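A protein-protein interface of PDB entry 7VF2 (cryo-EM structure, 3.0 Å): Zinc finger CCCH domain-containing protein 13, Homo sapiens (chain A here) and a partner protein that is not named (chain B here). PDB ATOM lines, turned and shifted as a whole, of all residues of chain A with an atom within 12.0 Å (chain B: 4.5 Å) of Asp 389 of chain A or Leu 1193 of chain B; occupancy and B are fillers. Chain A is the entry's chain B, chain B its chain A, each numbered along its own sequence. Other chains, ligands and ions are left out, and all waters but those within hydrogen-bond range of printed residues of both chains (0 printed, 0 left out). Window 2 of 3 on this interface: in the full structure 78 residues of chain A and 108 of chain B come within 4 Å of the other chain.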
ATOM      1  N   PRO A 387      -1.841  35.732  11.899  1.00  0.00           N
ATOM      2  CA  PRO A 387      -2.227  34.319  11.987  1.00  0.00           C
ATOM      3  C   PRO A 387      -3.414  33.988  11.093  1.00  0.00           C
ATOM      4  O   PRO A 387      -4.144  34.905  10.707  1.00  0.00           O
ATOM      5  CB  PRO A 387      -2.608  34.145  13.467  1.00  0.00           C
ATOM      6  CG  PRO A 387      -2.251  35.453  14.150  1.00  0.00           C
ATOM      7  CD  PRO A 387      -2.280  36.489  13.080  1.00  0.00           C
ATOM      8  N   LEU A 388      -3.613  32.701  10.794  1.00  0.00           N
ATOM      9  CA  LEU A 388      -4.781  32.260  10.038  1.00  0.00           C
ATOM     10  C   LEU A 388      -4.823  32.952   8.681  1.00  0.00           C
ATOM     11  O   LEU A 388      -5.681  33.805   8.438  1.00  0.00           O
ATOM     12  CB  LEU A 388      -6.065  32.512  10.833  1.00  0.00           C
ATOM     13  CG  LEU A 388      -6.184  31.723  12.142  1.00  0.00           C
ATOM     14  CD1 LEU A 388      -7.457  32.080  12.898  1.00  0.00           C
ATOM     15  CD2 LEU A 388      -6.099  30.227  11.889  1.00  0.00           C
ATOM     16  N   ASP A 389      -3.878  32.595   7.809  1.00  0.00           N
ATOM     17  CA  ASP A 389      -3.507  33.332   6.603  1.00  0.00           C
ATOM     18  C   ASP A 389      -4.687  33.848   5.783  1.00  0.00           C
ATOM     19  O   ASP A 389      -5.765  33.249   5.777  1.00  0.00           O
ATOM     20  CB  ASP A 389      -2.631  32.442   5.713  1.00  0.00           C
ATOM     21  CG  ASP A 389      -1.415  31.900   6.442  1.00  0.00           C
ATOM     22  OD1 ASP A 389      -1.403  30.689   6.751  1.00  0.00           O
ATOM     23  OD2 ASP A 389      -0.471  32.676   6.699  1.00  0.00           O
ATOM     24  N   VAL A 390      -4.488  34.972   5.093  1.00  0.00           N
ATOM     25  CA  VAL A 390      -5.515  35.567   4.251  1.00  0.00           C
ATOM     26  C   VAL A 390      -5.573  34.791   2.942  1.00  0.00           C
ATOM     27  O   VAL A 390      -4.554  34.530   2.299  1.00  0.00           O
ATOM     28  CB  VAL A 390      -5.264  37.068   3.986  1.00  0.00           C
ATOM     29  CG1 VAL A 390      -6.243  37.605   2.948  1.00  0.00           C
ATOM     30  CG2 VAL A 390      -5.371  37.858   5.284  1.00  0.00           C
ATOM     31  N   ILE A 391      -6.795  34.422   2.553  1.00  0.00           N
ATOM     32  CA  ILE A 391      -7.029  33.547   1.410  1.00  0.00           C
ATOM     33  C   ILE A 391      -7.865  34.266   0.358  1.00  0.00           C
ATOM     34  O   ILE A 391      -8.832  34.966   0.672  1.00  0.00           O
ATOM     35  CB  ILE A 391      -7.716  32.234   1.846  1.00  0.00           C
ATOM     36  CG1 ILE A 391      -8.031  31.365   0.632  1.00  0.00           C
ATOM     37  CG2 ILE A 391      -8.977  32.519   2.649  1.00  0.00           C
ATOM     38  CD1 ILE A 391      -8.577  30.018   0.991  1.00  0.00           C
ATOM     39  N   ASP A 392      -7.480  34.081  -0.906  1.00  0.00           N
ATOM     40  CA  ASP A 392      -8.254  34.536  -2.053  1.00  0.00           C
ATOM     41  C   ASP A 392      -8.214  33.467  -3.136  1.00  0.00           C
ATOM     42  O   ASP A 392      -7.302  32.641  -3.189  1.00  0.00           O
ATOM     43  CB  ASP A 392      -7.742  35.873  -2.607  1.00  0.00           C
ATOM     44  CG  ASP A 392      -8.144  37.055  -1.750  1.00  0.00           C
ATOM     45  OD1 ASP A 392      -9.218  36.994  -1.119  1.00  0.00           O
ATOM     46  OD2 ASP A 392      -7.395  38.052  -1.717  1.00  0.00           O
ATOM     47  N   VAL A 393      -9.213  33.507  -4.014  1.00  0.00           N
ATOM     48  CA  VAL A 393      -9.440  32.469  -5.016  1.00  0.00           C
ATOM     49  C   VAL A 393      -9.379  33.103  -6.402  1.00  0.00           C
ATOM     50  O   VAL A 393      -9.772  34.260  -6.577  1.00  0.00           O
ATOM     51  CB  VAL A 393     -10.785  31.755  -4.769  1.00  0.00           C
ATOM     52  CG1 VAL A 393     -11.907  32.760  -4.655  1.00  0.00           C
ATOM     53  CG2 VAL A 393     -11.084  30.754  -5.859  1.00  0.00           C
ATOM     54  N   SER B1189      -4.938  26.663   3.695  1.00  0.00           N
ATOM     55  CA  SER B1189      -4.101  27.005   4.843  1.00  0.00           C
ATOM     56  C   SER B1189      -4.872  27.629   5.997  1.00  0.00           C
ATOM     57  O   SER B1189      -4.620  27.245   7.152  1.00  0.00           O
ATOM     58  CB  SER B1189      -2.960  27.922   4.395  1.00  0.00           C
ATOM     59  OG  SER B1189      -2.455  28.679   5.483  1.00  0.00           O
ATOM     60  N   PRO B1190      -5.770  28.599   5.786  1.00  0.00           N
ATOM     61  CA  PRO B1190      -6.452  29.203   6.946  1.00  0.00           C
ATOM     62  C   PRO B1190      -7.190  28.194   7.809  1.00  0.00           C
ATOM     63  O   PRO B1190      -6.980  28.154   9.026  1.00  0.00           O
ATOM     64  CB  PRO B1190      -7.411  30.206   6.297  1.00  0.00           C
ATOM     65  CG  PRO B1190      -6.810  30.504   4.983  1.00  0.00           C
ATOM     66  CD  PRO B1190      -6.188  29.238   4.528  1.00  0.00           C
ATOM     67  N   THR B1191      -8.041  27.361   7.209  1.00  0.00           N
ATOM     68  CA  THR B1191      -8.802  26.394   7.991  1.00  0.00           C
ATOM     69  C   THR B1191      -7.924  25.273   8.535  1.00  0.00           C
ATOM     70  O   THR B1191      -8.202  24.745   9.620  1.00  0.00           O
ATOM     71  CB  THR B1191      -9.948  25.829   7.149  1.00  0.00           C
ATOM     72  OG1 THR B1191     -10.737  24.944   7.946  1.00  0.00           O
ATOM     73  CG2 THR B1191      -9.420  25.093   5.939  1.00  0.00           C
ATOM     74  N   ALA B1192      -6.852  24.916   7.825  1.00  0.00           N
ATOM     75  CA  ALA B1192      -5.908  23.935   8.351  1.00  0.00           C
ATOM     76  C   ALA B1192      -5.264  24.436   9.632  1.00  0.00           C
ATOM     77  O   ALA B1192      -5.253  23.737  10.654  1.00  0.00           O
ATOM     78  CB  ALA B1192      -4.835  23.621   7.314  1.00  0.00           C
ATOM     79  N   LEU B1193      -4.718  25.651   9.590  1.00  0.00           N
ATOM     80  CA  LEU B1193      -4.119  26.221  10.787  1.00  0.00           C
ATOM     81  C   LEU B1193      -5.164  26.443  11.866  1.00  0.00           C
ATOM     82  O   LEU B1193      -4.864  26.318  13.050  1.00  0.00           O
ATOM     83  CB  LEU B1193      -3.399  27.523  10.451  1.00  0.00           C
ATOM     84  CG  LEU B1193      -2.042  27.339   9.780  1.00  0.00           C
ATOM     85  CD1 LEU B1193      -1.514  28.670   9.293  1.00  0.00           C
ATOM     86  CD2 LEU B1193      -1.064  26.687  10.737  1.00  0.00           C
ATOM     87  N   LEU B1194      -6.405  26.739  11.482  1.00  0.00           N
ATOM     88  CA  LEU B1194      -7.469  26.889  12.469  1.00  0.00           C
ATOM     89  C   LEU B1194      -7.677  25.600  13.254  1.00  0.00           C
ATOM     90  O   LEU B1194      -7.617  25.584  14.490  1.00  0.00           O
ATOM     91  CB  LEU B1194      -8.760  27.311  11.770  1.00  0.00           C
ATOM     92  CG  LEU B1194     -10.029  27.303  12.612  1.00  0.00           C
ATOM     93  CD1 LEU B1194     -10.063  28.538  13.473  1.00  0.00           C
ATOM     94  CD2 LEU B1194     -11.250  27.239  11.721  1.00  0.00           C
ATOM     95  N   ILE B1195      -7.914  24.500  12.536  1.00  0.00           N
ATOM     96  CA  ILE B1195      -8.157  23.216  13.190  1.00  0.00           C
ATOM     97  C   ILE B1195      -6.955  22.800  14.024  1.00  0.00           C
ATOM     98  O   ILE B1195      -7.100  22.319  15.156  1.00  0.00           O
ATOM     99  CB  ILE B1195      -8.515  22.145  12.145  1.00  0.00           C
ATOM    100  CG1 ILE B1195      -9.887  22.432  11.553  1.00  0.00           C
ATOM    101  CG2 ILE B1195      -8.492  20.768  12.764  1.00  0.00           C
ATOM    102  CD1 ILE B1195     -10.959  22.623  12.588  1.00  0.00           C
ATOM    103  N   MET B1196      -5.748  22.986  13.490  1.00  0.00           N
ATOM    104  CA  MET B1196      -4.581  22.490  14.210  1.00  0.00           C
ATOM    105  C   MET B1196      -4.242  23.365  15.405  1.00  0.00           C
ATOM    106  O   MET B1196      -3.835  22.851  16.452  1.00  0.00           O
ATOM    107  CB  MET B1196      -3.393  22.357  13.271  1.00  0.00           C
ATOM    108  CG  MET B1196      -3.316  20.974  12.703  1.00  0.00           C
ATOM    109  SD  MET B1196      -3.340  19.801  14.065  1.00  0.00           S
ATOM    110  CE  MET B1196      -3.572  18.277  13.174  1.00  0.00           C
ATOM    111  N   ARG B1197      -4.406  24.684  15.284  1.00  0.00           N
ATOM    112  CA  ARG B1197      -4.279  25.542  16.450  1.00  0.00           C
ATOM    113  C   ARG B1197      -5.287  25.155  17.513  1.00  0.00           C
ATOM    114  O   ARG B1197      -4.968  25.168  18.701  1.00  0.00           O
ATOM    115  CB  ARG B1197      -4.463  27.008  16.070  1.00  0.00           C
ATOM    116  CG  ARG B1197      -3.304  27.623  15.328  1.00  0.00           C
ATOM    117  CD  ARG B1197      -3.687  28.987  14.794  1.00  0.00           C
ATOM    118  NE  ARG B1197      -3.539  30.017  15.812  1.00  0.00           N
ATOM    119  CZ  ARG B1197      -2.402  30.657  16.059  1.00  0.00           C
ATOM    120  NH1 ARG B1197      -1.318  30.370  15.353  1.00  0.00           N
ATOM    121  NH2 ARG B1197      -2.348  31.582  17.007  1.00  0.00           N
ATOM    122  N   ALA B1241       0.254  21.667   8.893  1.00  0.00           N
ATOM    123  CA  ALA B1241      -0.297  22.662   9.803  1.00  0.00           C
ATOM    124  C   ALA B1241       0.307  22.533  11.192  1.00  0.00           C
ATOM    125  O   ALA B1241       0.419  23.530  11.910  1.00  0.00           O
ATOM    126  CB  ALA B1241      -1.818  22.539   9.865  1.00  0.00           C
ATOM    127  N   LEU B1245       3.295  25.345  13.040  1.00  0.00           N
ATOM    128  CA  LEU B1245       3.039  25.850  14.381  1.00  0.00           C
ATOM    129  C   LEU B1245       4.153  25.528  15.359  1.00  0.00           C
ATOM    130  O   LEU B1245       4.436  26.337  16.242  1.00  0.00           O
ATOM    131  CB  LEU B1245       1.724  25.278  14.926  1.00  0.00           C
ATOM    132  CG  LEU B1245       0.454  25.695  14.188  1.00  0.00           C
ATOM    133  CD1 LEU B1245      -0.743  24.908  14.674  1.00  0.00           C
ATOM    134  CD2 LEU B1245       0.215  27.178  14.350  1.00  0.00           C
ATOM    135  N   LEU B1508       2.756  28.169   4.545  1.00  0.00           N
ATOM    136  CA  LEU B1508       1.768  27.108   4.375  1.00  0.00           C
ATOM    137  C   LEU B1508       0.786  27.438   3.260  1.00  0.00           C
ATOM    138  O   LEU B1508       0.307  26.539   2.558  1.00  0.00           O
ATOM    139  CB  LEU B1508       1.034  26.867   5.692  1.00  0.00           C
ATOM    140  CG  LEU B1508       0.165  25.614   5.744  1.00  0.00           C
ATOM    141  CD1 LEU B1508       0.951  24.418   5.256  1.00  0.00           C
ATOM    142  CD2 LEU B1508      -0.334  25.377   7.151  1.00  0.00           C
ATOM    143  N   GLN B1509       0.479  28.723   3.075  1.00  0.00           N
ATOM    144  CA  GLN B1509      -0.383  29.119   1.968  1.00  0.00           C
ATOM    145  C   GLN B1509       0.232  28.754   0.625  1.00  0.00           C
ATOM    146  O   GLN B1509      -0.480  28.323  -0.288  1.00  0.00           O
ATOM    147  CB  GLN B1509      -0.666  30.618   2.034  1.00  0.00           C
ATOM    148  CG  GLN B1509      -1.665  31.106   1.005  1.00  0.00           C
ATOM    149  CD  GLN B1509      -3.039  30.494   1.191  1.00  0.00           C
ATOM    150  OE1 GLN B1509      -3.829  30.957   2.014  1.00  0.00           O
ATOM    151  NE2 GLN B1509      -3.334  29.450   0.425  1.00  0.00           N
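O of Pro 1190 of chain B touches CD2 of Leu 388 of chain A (3.6 Å). Leu 1193 of chain B touches Leu 388 of chain A (C to CD2, 3.9 Å). Leu 388 of chain A touches Leu 1194 of chain B. Leu 388 of chain A touches Arg 1197 of chain B. CG of Pro 1190 of chain B touches O of Asp 389 of chain A, 3.0 Å away. Asp 389 of chain A touches Leu 1193 of chain B. Val 390 of chain A touches Gln 1509 of chain B. CG of Pro 1190 of chain B touches CB of Ile 391 of chain A, 3.7 Å away.
Hydrophobic or aromatic side chains of chain A that line the printed part of chain B: Leu 388 and Ile 391. Of the 13 printed residues of chain B, 6 touch a printed residue of chain A. Printed residues of chain B that touch a printed residue of chain A: Ser 1189, Pro 1190, Leu 1193, Leu 1194, Arg 1197 and Gln 1509. Hydrophobic or aromatic side chains of chain B that line the printed part of chain A: Pro 1190, Leu 1193 and Leu 1194. Among the printed residues, 9 pairs touch across the chains. Among the printed residues, no Asp or Glu carboxylate lies within 4 Å of a Lys or Arg side-chain nitrogen of the other chain.
Printed residues of chain B within 4 Å of Leu 388 of chain A: Pro 1190, Leu 1193, Leu 1194 and Arg 1197. Of chain B, only Ser 1189, Pro 1190 and Leu 1193 come within 4 Å of Asp 389 of chain A. Printed residues of chain B within 4 Å of Val 390 of chain A: Gln 1509. Printed residues of chain B within 4 Å of Ile 391 of chain A: Pro 1190. Asp 392 of chain A touches none of the printed residues of chain B. Of chain A, only Asp 389 (2.6 Å) comes within 4 Å of Ser 1189 of chain B. Pro 1190 of chain B touches just these residues of chain A: Leu 388 (3.6 Å), Asp 389 (3.0 Å) and Ile 391 (3.7 Å). No residue of chain A comes within 4 Å of Thr 1191 of chain B. No residue of chain A comes within 4 Å of Ala 1192 of chain B. Of chain A, only Leu 388 and Asp 389 come within 4 Å of Leu 1193 of chain B. Of the printed residues of chain A, Leu 1194 of chain B touches Leu 388. Ile 1195 of chain B touches none of the printed residues of chain A. Met 1196 of chain B touches none of the printed residues of chain A. Of chain A, only Leu 388 (3.97 Å) comes within 4 Å of Arg 1197 of chain B. No residue of chain A comes within 4 Å of Leu 1245 of chain B. Gln 1509 of chain B touches just one residue of chain A: Val 390.
The side-chain hydroxyl of Ser 1189 of chain B is in hydrogen-bond range of the side-chain carboxylate of Asp 389 of chain A, 2.6 Å away.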
